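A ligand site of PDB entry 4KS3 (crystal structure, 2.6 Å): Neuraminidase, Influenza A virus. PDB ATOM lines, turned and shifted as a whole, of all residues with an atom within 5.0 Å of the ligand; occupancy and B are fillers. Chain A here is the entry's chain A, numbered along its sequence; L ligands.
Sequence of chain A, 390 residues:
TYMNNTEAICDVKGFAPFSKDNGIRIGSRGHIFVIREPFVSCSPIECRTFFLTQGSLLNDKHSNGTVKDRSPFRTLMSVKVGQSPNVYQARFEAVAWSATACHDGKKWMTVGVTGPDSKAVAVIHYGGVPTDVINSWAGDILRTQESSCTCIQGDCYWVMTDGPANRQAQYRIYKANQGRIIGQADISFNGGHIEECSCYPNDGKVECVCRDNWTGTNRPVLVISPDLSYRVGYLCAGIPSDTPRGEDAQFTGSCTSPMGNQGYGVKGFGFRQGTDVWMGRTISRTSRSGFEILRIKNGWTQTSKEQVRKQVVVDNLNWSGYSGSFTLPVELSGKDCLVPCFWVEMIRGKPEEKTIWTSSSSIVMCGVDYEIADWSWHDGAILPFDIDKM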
ATOM      1  N   ARG A  36       6.739   4.030 -27.543  1.00  0.00           N
ATOM      2  CA  ARG A  36       5.439   4.584 -27.889  1.00  0.00           C
ATOM      3  C   ARG A  36       5.731   5.983 -28.416  1.00  0.00           C
ATOM      4  O   ARG A  36       6.892   6.344 -28.632  1.00  0.00           O
ATOM      5  CB  ARG A  36       4.510   4.665 -26.673  1.00  0.00           C
ATOM      6  CG  ARG A  36       3.819   3.360 -26.280  1.00  0.00           C
ATOM      7  CD  ARG A  36       2.431   3.201 -26.896  1.00  0.00           C
ATOM      8  NE  ARG A  36       1.814   4.483 -27.240  1.00  0.00           N
ATOM      9  CZ  ARG A  36       0.862   5.095 -26.531  1.00  0.00           C
ATOM     10  NH1 ARG A  36       0.393   6.248 -26.947  1.00  0.00           N
ATOM     11  NH2 ARG A  36       0.387   4.570 -25.415  1.00  0.00           N
ATOM     12  N   GLU A  37       4.684   6.771 -28.607  1.00  0.00           N
ATOM     13  CA  GLU A  37       4.806   8.143 -29.128  1.00  0.00           C
ATOM     14  C   GLU A  37       5.841   8.354 -30.231  1.00  0.00           C
ATOM     15  O   GLU A  37       6.693   9.230 -30.117  1.00  0.00           O
ATOM     16  CB  GLU A  37       5.087   9.116 -27.985  1.00  0.00           C
ATOM     17  CG  GLU A  37       3.994   9.184 -26.939  1.00  0.00           C
ATOM     18  CD  GLU A  37       4.040   8.026 -25.972  1.00  0.00           C
ATOM     19  OE1 GLU A  37       5.151   7.566 -25.653  1.00  0.00           O
ATOM     20  OE2 GLU A  37       2.961   7.587 -25.527  1.00  0.00           O
ATOM     21  N   LEU A  52      10.004   7.425 -28.135  1.00  0.00           N
ATOM     22  CA  LEU A  52      10.346   7.282 -26.738  1.00  0.00           C
ATOM     23  C   LEU A  52      10.550   5.822 -26.422  1.00  0.00           C
ATOM     24  O   LEU A  52       9.600   5.054 -26.402  1.00  0.00           O
ATOM     25  CB  LEU A  52       9.225   7.811 -25.855  1.00  0.00           C
ATOM     26  CG  LEU A  52       8.776   9.242 -26.087  1.00  0.00           C
ATOM     27  CD1 LEU A  52       7.610   9.561 -25.158  1.00  0.00           C
ATOM     28  CD2 LEU A  52       9.925  10.219 -25.880  1.00  0.00           C
ATOM     29  N   GLN A  54      11.402   2.610 -24.055  1.00  0.00           N
ATOM     30  CA  GLN A  54      11.118   2.238 -22.689  1.00  0.00           C
ATOM     31  C   GLN A  54      12.390   1.722 -22.060  1.00  0.00           C
ATOM     32  O   GLN A  54      12.352   0.908 -21.137  1.00  0.00           O
ATOM     33  CB  GLN A  54      10.042   1.171 -22.626  1.00  0.00           C
ATOM     34  CG  GLN A  54       8.676   1.715 -22.306  1.00  0.00           C
ATOM     35  CD  GLN A  54       8.660   2.483 -20.997  1.00  0.00           C
ATOM     36  OE1 GLN A  54       9.521   2.304 -20.135  1.00  0.00           O
ATOM     37  NE2 GLN A  54       7.678   3.352 -20.845  1.00  0.00           N
ATOM     38  N   THR A  66       5.666  -2.226 -19.665  1.00  0.00           N
ATOM     39  CA  THR A  66       5.985  -1.089 -20.517  1.00  0.00           C
ATOM     40  C   THR A  66       4.732  -0.328 -21.004  1.00  0.00           C
ATOM     41  O   THR A  66       4.790   0.446 -21.968  1.00  0.00           O
ATOM     42  CB  THR A  66       6.911  -1.455 -21.690  1.00  0.00           C
ATOM     43  OG1 THR A  66       6.463  -2.681 -22.273  1.00  0.00           O
ATOM     44  CG2 THR A  66       8.339  -1.634 -21.191  1.00  0.00           C
ATOM     45  N   VAL A  67       3.616  -0.556 -20.313  1.00  0.00           N
ATOM     46  CA  VAL A  67       2.392   0.182 -20.547  1.00  0.00           C
ATOM     47  C   VAL A  67       2.373   1.451 -19.697  1.00  0.00           C
ATOM     48  O   VAL A  67       1.678   2.420 -20.013  1.00  0.00           O
ATOM     49  CB  VAL A  67       1.165  -0.683 -20.228  1.00  0.00           C
ATOM     50  CG1 VAL A  67       1.059  -0.941 -18.739  1.00  0.00           C
ATOM     51  CG2 VAL A  67      -0.099  -0.021 -20.729  1.00  0.00           C
ATOM     52  N   LYS A  68       3.155   1.442 -18.612  1.00  0.00           N
ATOM     53  CA  LYS A  68       3.336   2.609 -17.764  1.00  0.00           C
ATOM     54  C   LYS A  68       3.762   3.786 -18.623  1.00  0.00           C
ATOM     55  O   LYS A  68       4.325   3.594 -19.703  1.00  0.00           O
ATOM     56  CB  LYS A  68       4.393   2.349 -16.688  1.00  0.00           C
ATOM     57  CG  LYS A  68       3.925   1.408 -15.588  1.00  0.00           C
ATOM     58  CD  LYS A  68       4.945   1.311 -14.454  1.00  0.00           C
ATOM     59  CE  LYS A  68       4.436   0.420 -13.336  1.00  0.00           C
ATOM     60  NZ  LYS A  68       5.370   0.334 -12.173  1.00  0.00           N
ATOM     61  N   ASP A  69       3.486   5.007 -18.167  1.00  0.00           N
ATOM     62  CA  ASP A  69       3.756   6.177 -18.993  1.00  0.00           C
ATOM     63  C   ASP A  69       5.095   6.829 -18.723  1.00  0.00           C
ATOM     64  O   ASP A  69       5.810   7.217 -19.651  1.00  0.00           O
ATOM     65  CB  ASP A  69       2.608   7.180 -18.911  1.00  0.00           C
ATOM     66  CG  ASP A  69       1.334   6.649 -19.541  1.00  0.00           C
ATOM     67  OD1 ASP A  69       1.414   5.970 -20.585  1.00  0.00           O
ATOM     68  OD2 ASP A  69       0.237   6.902 -18.988  1.00  0.00           O
ATOM     69  N   ARG A  70       5.459   6.957 -17.453  1.00  0.00           N
ATOM     70  CA  ARG A  70       6.622   7.762 -17.109  1.00  0.00           C
ATOM     71  C   ARG A  70       7.607   7.005 -16.216  1.00  0.00           C
ATOM     72  O   ARG A  70       7.368   6.825 -15.019  1.00  0.00           O
ATOM     73  CB  ARG A  70       6.177   9.091 -16.478  1.00  0.00           C
ATOM     74  CG  ARG A  70       5.154   9.860 -17.353  1.00  0.00           C
ATOM     75  CD  ARG A  70       4.443  11.010 -16.623  1.00  0.00           C
ATOM     76  NE  ARG A  70       3.589  10.537 -15.547  1.00  0.00           N
ATOM     77  CZ  ARG A  70       2.315  10.180 -15.681  1.00  0.00           C
ATOM     78  NH1 ARG A  70       1.631   9.767 -14.620  1.00  0.00           N
ATOM     79  NH2 ARG A  70       1.709  10.241 -16.858  1.00  0.00           N
ATOM     80  N   ARG A  74      13.212   6.200 -19.587  1.00  0.00           N
ATOM     81  CA  ARG A  74      12.611   6.691 -20.802  1.00  0.00           C
ATOM     82  C   ARG A  74      13.539   7.658 -21.511  1.00  0.00           C
ATOM     83  O   ARG A  74      14.032   8.599 -20.894  1.00  0.00           O
ATOM     84  CB  ARG A  74      11.314   7.391 -20.451  1.00  0.00           C
ATOM     85  CG  ARG A  74      10.251   7.213 -21.461  1.00  0.00           C
ATOM     86  CD  ARG A  74       9.645   5.868 -21.359  1.00  0.00           C
ATOM     87  NE  ARG A  74       8.911   5.610 -22.579  1.00  0.00           N
ATOM     88  CZ  ARG A  74       7.746   6.177 -22.847  1.00  0.00           C
ATOM     89  NH1 ARG A  74       7.118   5.897 -23.986  1.00  0.00           N
ATOM     90  NH2 ARG A  74       7.204   7.016 -21.971  1.00  0.00           N
ATOM     91  N   TRP A  97      10.015  11.255 -21.157  1.00  0.00           N
ATOM     92  CA  TRP A  97       8.779  10.483 -21.214  1.00  0.00           C
ATOM     93  C   TRP A  97       7.641  11.315 -21.822  1.00  0.00           C
ATOM     94  O   TRP A  97       6.488  10.917 -21.811  1.00  0.00           O
ATOM     95  CB  TRP A  97       8.389   9.889 -19.849  1.00  0.00           C
ATOM     96  CG  TRP A  97       8.622  10.782 -18.645  1.00  0.00           C
ATOM     97  CD1 TRP A  97       9.549  10.597 -17.677  1.00  0.00           C
ATOM     98  CD2 TRP A  97       7.900  11.966 -18.290  1.00  0.00           C
ATOM     99  NE1 TRP A  97       9.458  11.595 -16.738  1.00  0.00           N
ATOM    100  CE2 TRP A  97       8.453  12.448 -17.092  1.00  0.00           C
ATOM    101  CE3 TRP A  97       6.839  12.675 -18.873  1.00  0.00           C
ATOM    102  CZ2 TRP A  97       7.984  13.601 -16.453  1.00  0.00           C
ATOM    103  CZ3 TRP A  97       6.372  13.822 -18.242  1.00  0.00           C
ATOM    104  CH2 TRP A  97       6.951  14.272 -17.040  1.00  0.00           C
ATOM    105  N   SER A  98       8.010  12.487 -22.342  1.00  0.00           N
ATOM    106  CA  SER A  98       7.152  13.344 -23.154  1.00  0.00           C
ATOM    107  C   SER A  98       8.081  14.254 -23.973  1.00  0.00           C
ATOM    108  O   SER A  98       9.076  14.753 -23.449  1.00  0.00           O
ATOM    109  CB  SER A  98       6.196  14.160 -22.284  1.00  0.00           C
ATOM    110  OG  SER A  98       5.328  14.965 -23.066  1.00  0.00           O
ATOM    111  N   ILE A 141       2.752  16.932 -13.829  1.00  0.00           N
ATOM    112  CA  ILE A 141       3.056  16.261 -15.106  1.00  0.00           C
ATOM    113  C   ILE A 141       3.336  17.161 -16.330  1.00  0.00           C
ATOM    114  O   ILE A 141       2.735  16.973 -17.386  1.00  0.00           O
ATOM    115  CB  ILE A 141       1.979  15.235 -15.493  1.00  0.00           C
ATOM    116  CG1 ILE A 141       1.692  14.280 -14.334  1.00  0.00           C
ATOM    117  CG2 ILE A 141       2.394  14.466 -16.738  1.00  0.00           C
ATOM    118  CD1 ILE A 141       0.866  13.074 -14.720  1.00  0.00           C
ATOM    119  N   ARG A 143       4.255  18.451 -19.679  1.00  0.00           N
ATOM    120  CA  ARG A 143       4.232  17.620 -20.863  1.00  0.00           C
ATOM    121  C   ARG A 143       4.037  18.439 -22.133  1.00  0.00           C
ATOM    122  O   ARG A 143       3.726  19.636 -22.071  1.00  0.00           O
ATOM    123  CB  ARG A 143       3.144  16.570 -20.729  1.00  0.00           C
ATOM    124  CG  ARG A 143       1.826  17.139 -20.302  1.00  0.00           C
ATOM    125  CD  ARG A 143       0.957  16.087 -19.645  1.00  0.00           C
ATOM    126  NE  ARG A 143      -0.416  16.560 -19.536  1.00  0.00           N
ATOM    127  CZ  ARG A 143      -0.868  17.280 -18.525  1.00  0.00           C
ATOM    128  NH1 ARG A 143      -2.129  17.684 -18.512  1.00  0.00           N
ATOM    129  NH2 ARG A 143      -0.064  17.593 -17.514  1.00  0.00           N
ATOM    130  N   GLU A 146       4.547  15.471 -28.352  1.00  0.00           N
ATOM    131  CA  GLU A 146       4.758  14.110 -28.872  1.00  0.00           C
ATOM    132  C   GLU A 146       4.587  14.059 -30.379  1.00  0.00           C
ATOM    133  O   GLU A 146       4.208  13.021 -30.939  1.00  0.00           O
ATOM    134  CB  GLU A 146       3.839  13.076 -28.192  1.00  0.00           C
ATOM    135  CG  GLU A 146       3.353  13.415 -26.795  1.00  0.00           C
ATOM    136  CD  GLU A 146       4.404  13.283 -25.727  1.00  0.00           C
ATOM    137  OE1 GLU A 146       5.611  13.224 -26.032  1.00  0.00           O
ATOM    138  OE2 GLU A 146       3.994  13.221 -24.543  1.00  0.00           O
ATOM    139  N   ALA A 165      -5.227  16.148 -15.521  1.00  0.00           N
ATOM    140  CA  ALA A 165      -5.480  15.462 -16.775  1.00  0.00           C
ATOM    141  C   ALA A 165      -6.913  15.638 -17.261  1.00  0.00           C
ATOM    142  O   ALA A 165      -7.147  15.665 -18.459  1.00  0.00           O
ATOM    143  CB  ALA A 165      -5.129  13.994 -16.643  1.00  0.00           C
ATOM    144  N   GLU A 195      -4.097  19.590 -25.272  1.00  0.00           N
ATOM    145  CA  GLU A 195      -2.989  18.659 -25.107  1.00  0.00           C
ATOM    146  C   GLU A 195      -2.501  18.129 -26.458  1.00  0.00           C
ATOM    147  O   GLU A 195      -3.245  18.111 -27.430  1.00  0.00           O
ATOM    148  CB  GLU A 195      -3.386  17.478 -24.213  1.00  0.00           C
ATOM    149  CG  GLU A 195      -3.316  17.770 -22.728  1.00  0.00           C
ATOM    150  CD  GLU A 195      -3.550  16.535 -21.888  1.00  0.00           C
ATOM    151  OE1 GLU A 195      -3.909  15.502 -22.469  1.00  0.00           O
ATOM    152  OE2 GLU A 195      -3.378  16.611 -20.651  1.00  0.00           O
ATOM    153  N   GLU A 196      -1.239  17.706 -26.483  1.00  0.00           N
ATOM    154  CA  GLU A 196      -0.630  16.995 -27.613  1.00  0.00           C
ATOM    155  C   GLU A 196      -0.924  17.617 -28.969  1.00  0.00           C
ATOM    156  O   GLU A 196      -1.507  16.961 -29.837  1.00  0.00           O
ATOM    157  CB  GLU A 196      -1.040  15.521 -27.570  1.00  0.00           C
ATOM    158  CG  GLU A 196      -0.432  14.764 -26.381  1.00  0.00           C
ATOM    159  CD  GLU A 196      -1.096  13.424 -26.129  1.00  0.00           C
ATOM    160  OE1 GLU A 196      -2.191  13.179 -26.670  1.00  0.00           O
ATOM    161  OE2 GLU A 196      -0.524  12.609 -25.375  1.00  0.00           O
ATOM    162  N   ARG A 211      -5.456  18.108 -28.374  1.00  0.00           N
ATOM    163  CA  ARG A 211      -6.391  17.153 -27.783  1.00  0.00           C
ATOM    164  C   ARG A 211      -7.099  17.657 -26.551  1.00  0.00           C
ATOM    165  O   ARG A 211      -6.473  18.251 -25.681  1.00  0.00           O
ATOM    166  CB  ARG A 211      -5.607  15.890 -27.441  1.00  0.00           C
ATOM    167  CG  ARG A 211      -6.271  14.975 -26.412  1.00  0.00           C
ATOM    168  CD  ARG A 211      -5.312  13.853 -26.037  1.00  0.00           C
ATOM    169  NE  ARG A 211      -5.869  12.881 -25.112  1.00  0.00           N
ATOM    170  CZ  ARG A 211      -5.236  11.765 -24.734  1.00  0.00           C
ATOM    171  NH1 ARG A 211      -5.815  10.926 -23.887  1.00  0.00           N
ATOM    172  NH2 ARG A 211      -4.031  11.484 -25.215  1.00  0.00           N
ATOM    173  N   ASN A 213      -8.756  16.475 -23.354  1.00  0.00           N
ATOM    174  CA  ASN A 213      -8.927  15.319 -22.498  1.00  0.00           C
ATOM    175  C   ASN A 213      -9.966  15.586 -21.416  1.00  0.00           C
ATOM    176  O   ASN A 213     -10.178  14.776 -20.520  1.00  0.00           O
ATOM    177  CB  ASN A 213      -7.591  14.905 -21.901  1.00  0.00           C
ATOM    178  CG  ASN A 213      -7.454  13.399 -21.770  1.00  0.00           C
ATOM    179  OD1 ASN A 213      -7.229  12.712 -22.768  1.00  0.00           O
ATOM    180  ND2 ASN A 213      -7.593  12.891 -20.558  1.00  0.00           N
ATOM    181  N   TYR A 264     -11.637  11.681 -21.598  1.00  0.00           N
ATOM    182  CA  TYR A 264     -10.531  11.041 -22.295  1.00  0.00           C
ATOM    183  C   TYR A 264     -10.195  11.737 -23.618  1.00  0.00           C
ATOM    184  O   TYR A 264     -10.611  12.869 -23.873  1.00  0.00           O
ATOM    185  CB  TYR A 264     -10.869   9.565 -22.522  1.00  0.00           C
ATOM    186  CG  TYR A 264      -9.764   8.692 -23.073  1.00  0.00           C
ATOM    187  CD1 TYR A 264      -8.451   9.146 -23.135  1.00  0.00           C
ATOM    188  CD2 TYR A 264     -10.035   7.409 -23.522  1.00  0.00           C
ATOM    189  CE1 TYR A 264      -7.441   8.332 -23.640  1.00  0.00           C
ATOM    190  CE2 TYR A 264      -9.040   6.593 -24.018  1.00  0.00           C
ATOM    191  CZ  TYR A 264      -7.744   7.064 -24.084  1.00  0.00           C
ATOM    192  OH  TYR A 264      -6.760   6.242 -24.580  1.00  0.00           O
ATOM    193  N   GLY A 265      -9.438  11.041 -24.450  1.00  0.00           N
ATOM    194  CA  GLY A 265      -9.038  11.566 -25.733  1.00  0.00           C
ATOM    195  C   GLY A 265      -7.906  10.768 -26.348  1.00  0.00           C
ATOM    196  O   GLY A 265      -7.412   9.796 -25.772  1.00  0.00           O
ATOM    197  N   ARG A 288      -9.291   2.352 -30.042  1.00  0.00           N
ATOM    198  CA  ARG A 288      -8.195   2.840 -30.841  1.00  0.00           C
ATOM    199  C   ARG A 288      -7.886   1.866 -31.964  1.00  0.00           C
ATOM    200  O   ARG A 288      -6.789   1.300 -32.019  1.00  0.00           O
ATOM    201  CB  ARG A 288      -6.965   3.052 -29.963  1.00  0.00           C
ATOM    202  CG  ARG A 288      -7.166   4.166 -28.971  1.00  0.00           C
ATOM    203  CD  ARG A 288      -5.949   4.345 -28.076  1.00  0.00           C
ATOM    204  NE  ARG A 288      -5.943   5.672 -27.485  1.00  0.00           N
ATOM    205  CZ  ARG A 288      -4.973   6.167 -26.736  1.00  0.00           C
ATOM    206  NH1 ARG A 288      -5.081   7.394 -26.261  1.00  0.00           N
ATOM    207  NH2 ARG A 288      -3.895   5.453 -26.449  1.00  0.00           N
ATOM    208  N   TYR A 322      -2.218   7.101 -31.737  1.00  0.00           N
ATOM    209  CA  TYR A 322      -1.782   8.450 -32.071  1.00  0.00           C
ATOM    210  C   TYR A 322      -1.466   8.710 -33.539  1.00  0.00           C
ATOM    211  O   TYR A 322      -1.074   7.820 -34.279  1.00  0.00           O
ATOM    212  CB  TYR A 322      -0.478   8.772 -31.362  1.00  0.00           C
ATOM    213  CG  TYR A 322      -0.629   9.155 -29.911  1.00  0.00           C
ATOM    214  CD1 TYR A 322      -1.819   8.914 -29.232  1.00  0.00           C
ATOM    215  CD2 TYR A 322       0.408   9.772 -29.219  1.00  0.00           C
ATOM    216  CE1 TYR A 322      -1.966   9.275 -27.911  1.00  0.00           C
ATOM    217  CE2 TYR A 322       0.273  10.140 -27.899  1.00  0.00           C
ATOM    218  CZ  TYR A 322      -0.919   9.885 -27.249  1.00  0.00           C
ATOM    219  OH  TYR A 322      -1.060  10.263 -25.936  1.00  0.00           O
ATOM    220  N   THR A 358       3.795  -3.245 -24.084  1.00  0.00           N
ATOM    221  CA  THR A 358       3.064  -2.345 -24.949  1.00  0.00           C
ATOM    222  C   THR A 358       4.062  -1.613 -25.830  1.00  0.00           C
ATOM    223  O   THR A 358       5.085  -1.130 -25.361  1.00  0.00           O
ATOM    224  CB  THR A 358       2.287  -1.318 -24.135  1.00  0.00           C
ATOM    225  OG1 THR A 358       1.264  -1.975 -23.380  1.00  0.00           O
ATOM    226  CG2 THR A 358       1.665  -0.284 -25.053  1.00  0.00           C
HETATM  227  C1  LIG L   1      -4.048   9.578 -20.029  1.00  0.00           C
HETATM  228  C2  LIG L   1      -3.185  10.812 -19.698  1.00  0.00           C
HETATM  229  C3  LIG L   1      -2.682  11.551 -20.953  1.00  0.00           C
HETATM  230  C4  LIG L   1      -3.166  12.990 -20.897  1.00  0.00           C
HETATM  231  C5  LIG L   1      -2.308  13.819 -19.928  1.00  0.00           C
HETATM  232  O1  LIG L   1      -1.255  11.553 -20.955  1.00  0.00           O
HETATM  233  C6  LIG L   1      -0.690  10.850 -22.079  1.00  0.00           C
HETATM  234  C7  LIG L   1       0.707  10.342 -21.710  1.00  0.00           C
HETATM  235  N1  LIG L   1       1.564  11.486 -21.374  1.00  0.00           N
HETATM  236  C8  LIG L   1       2.464  11.471 -20.398  1.00  0.00           C
HETATM  237  C9  LIG L   1       3.360  12.702 -20.347  1.00  0.00           C
HETATM  238  O2  LIG L   1       2.604  10.533 -19.626  1.00  0.00           O
HETATM  239  C10 LIG L   1      -1.577   9.670 -22.437  1.00  0.00           C
HETATM  240  C11 LIG L   1      -0.916   8.600 -23.281  1.00  0.00           C
HETATM  241  C12 LIG L   1      -1.869   7.741 -24.101  1.00  0.00           C
HETATM  242  O3  LIG L   1      -1.420   6.708 -24.663  1.00  0.00           O
HETATM  243  O4  LIG L   1      -3.073   8.077 -24.041  1.00  0.00           O
HETATM  244  C13 LIG L   1       0.406   8.736 -23.675  1.00  0.00           C
HETATM  245  C14 LIG L   1       1.362   9.657 -22.917  1.00  0.00           C
HETATM  246  N2  LIG L   1       2.526   8.851 -22.560  1.00  0.00           N
HETATM  247  C15 LIG L   1       2.531   7.541 -22.697  1.00  0.00           C
HETATM  248  N3  LIG L   1       3.616   9.266 -22.151  1.00  0.00           N
HETATM  249  N4  LIG L   1       4.375   8.308 -21.995  1.00  0.00           N
HETATM  250  C16 LIG L   1       3.737   7.178 -22.327  1.00  0.00           C
HETATM  251  C17 LIG L   1       4.297   5.754 -22.322  1.00  0.00           C
HETATM  252  C18 LIG L   1       3.370   4.721 -22.954  1.00  0.00           C
HETATM  253  C19 LIG L   1       4.020   3.343 -22.795  1.00  0.00           C
HETATM  254  O5  LIG L   1       3.181   2.310 -23.293  1.00  0.00           O
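O2 of the ligand sits at hydrogen-bond distance from NH2 of Arg 70. NH1 of Arg 288 lies within salt-bridge range of O4 of the ligand. N4 of the ligand sits at hydrogen-bond distance from NH2 of Arg 74 (3.1 Å). An oxygen (O3) of the ligand is in salt-bridge range of the guanidinium group of Arg 36. O of Thr 66 sits at hydrogen-bond distance from O5 of the ligand, 2.8 Å away. The guanidinium group of Arg 211 lies within salt-bridge range of an oxygen (O4) of the ligand.
The side-chain amide oxygen of Asn 213 sits at hydrogen-bond distance from the guanidinium group of Arg 211 (2.5 Å). O of Gly 265 sits at hydrogen-bond distance from NH1 of Arg 288, 3.4 Å away. O of Asp 69 is in hydrogen-bond range of NH2 of Arg 74 (2.7 Å). The side-chain hydroxyl (OH) of Tyr 322 lies within hydrogen-bond range of the side-chain carboxylate (OE2) of Glu 196, at 2.5 Å. The side-chain hydroxyl (OG1) of Thr 66 is in hydrogen-bond range of the backbone NH (N) of Thr 358 (3.3 Å). The backbone carbonyl oxygen (O) of Gly 265 lies within hydrogen-bond range of the guanidinium group (NH1) of Arg 211, 2.7 Å away. The side-chain hydroxyl of Tyr 322 is in hydrogen-bond range of the guanidinium group of Arg 211. The guanidinium group (NH2) of Arg 211 lies within salt-bridge range of the side-chain carboxylate (OE1) of Glu 196 (2.9 Å).
A nitrogen (N2) of the ligand lies close to the side-chain carboxylate of Glu 37, 3.3 Å away. The backbone carbonyl oxygen (O) of Asp 69 sits close to a nitrogen (N4) of the ligand (3.0 Å). The backbone carbonyl oxygen of Trp 97 sits close to a nitrogen (N3) of the ligand (3.3 Å). Residues that only touch the ligand: Val 67 (3.6 Å), Lys 68 (3.1 Å), Ser 98 (3.7 Å), Arg 143 (3.4 Å), Glu 195 (3.1 Å), Glu 196 (3.7 Å), Tyr 322 (3.1 Å) and Thr 358 (3.5 Å). Hydrophobic or aromatic side chains that line the ligand: Trp 97 and Tyr 322. Within 4 Å of the ligand: Arg 36, Glu 37, Thr 66, Val 67, Lys 68, Asp 69, Arg 70, Arg 74, Trp 97, Ser 98, Arg 143, Glu 195, Glu 196, Arg 211, Arg 288, Tyr 322 and Thr 358.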
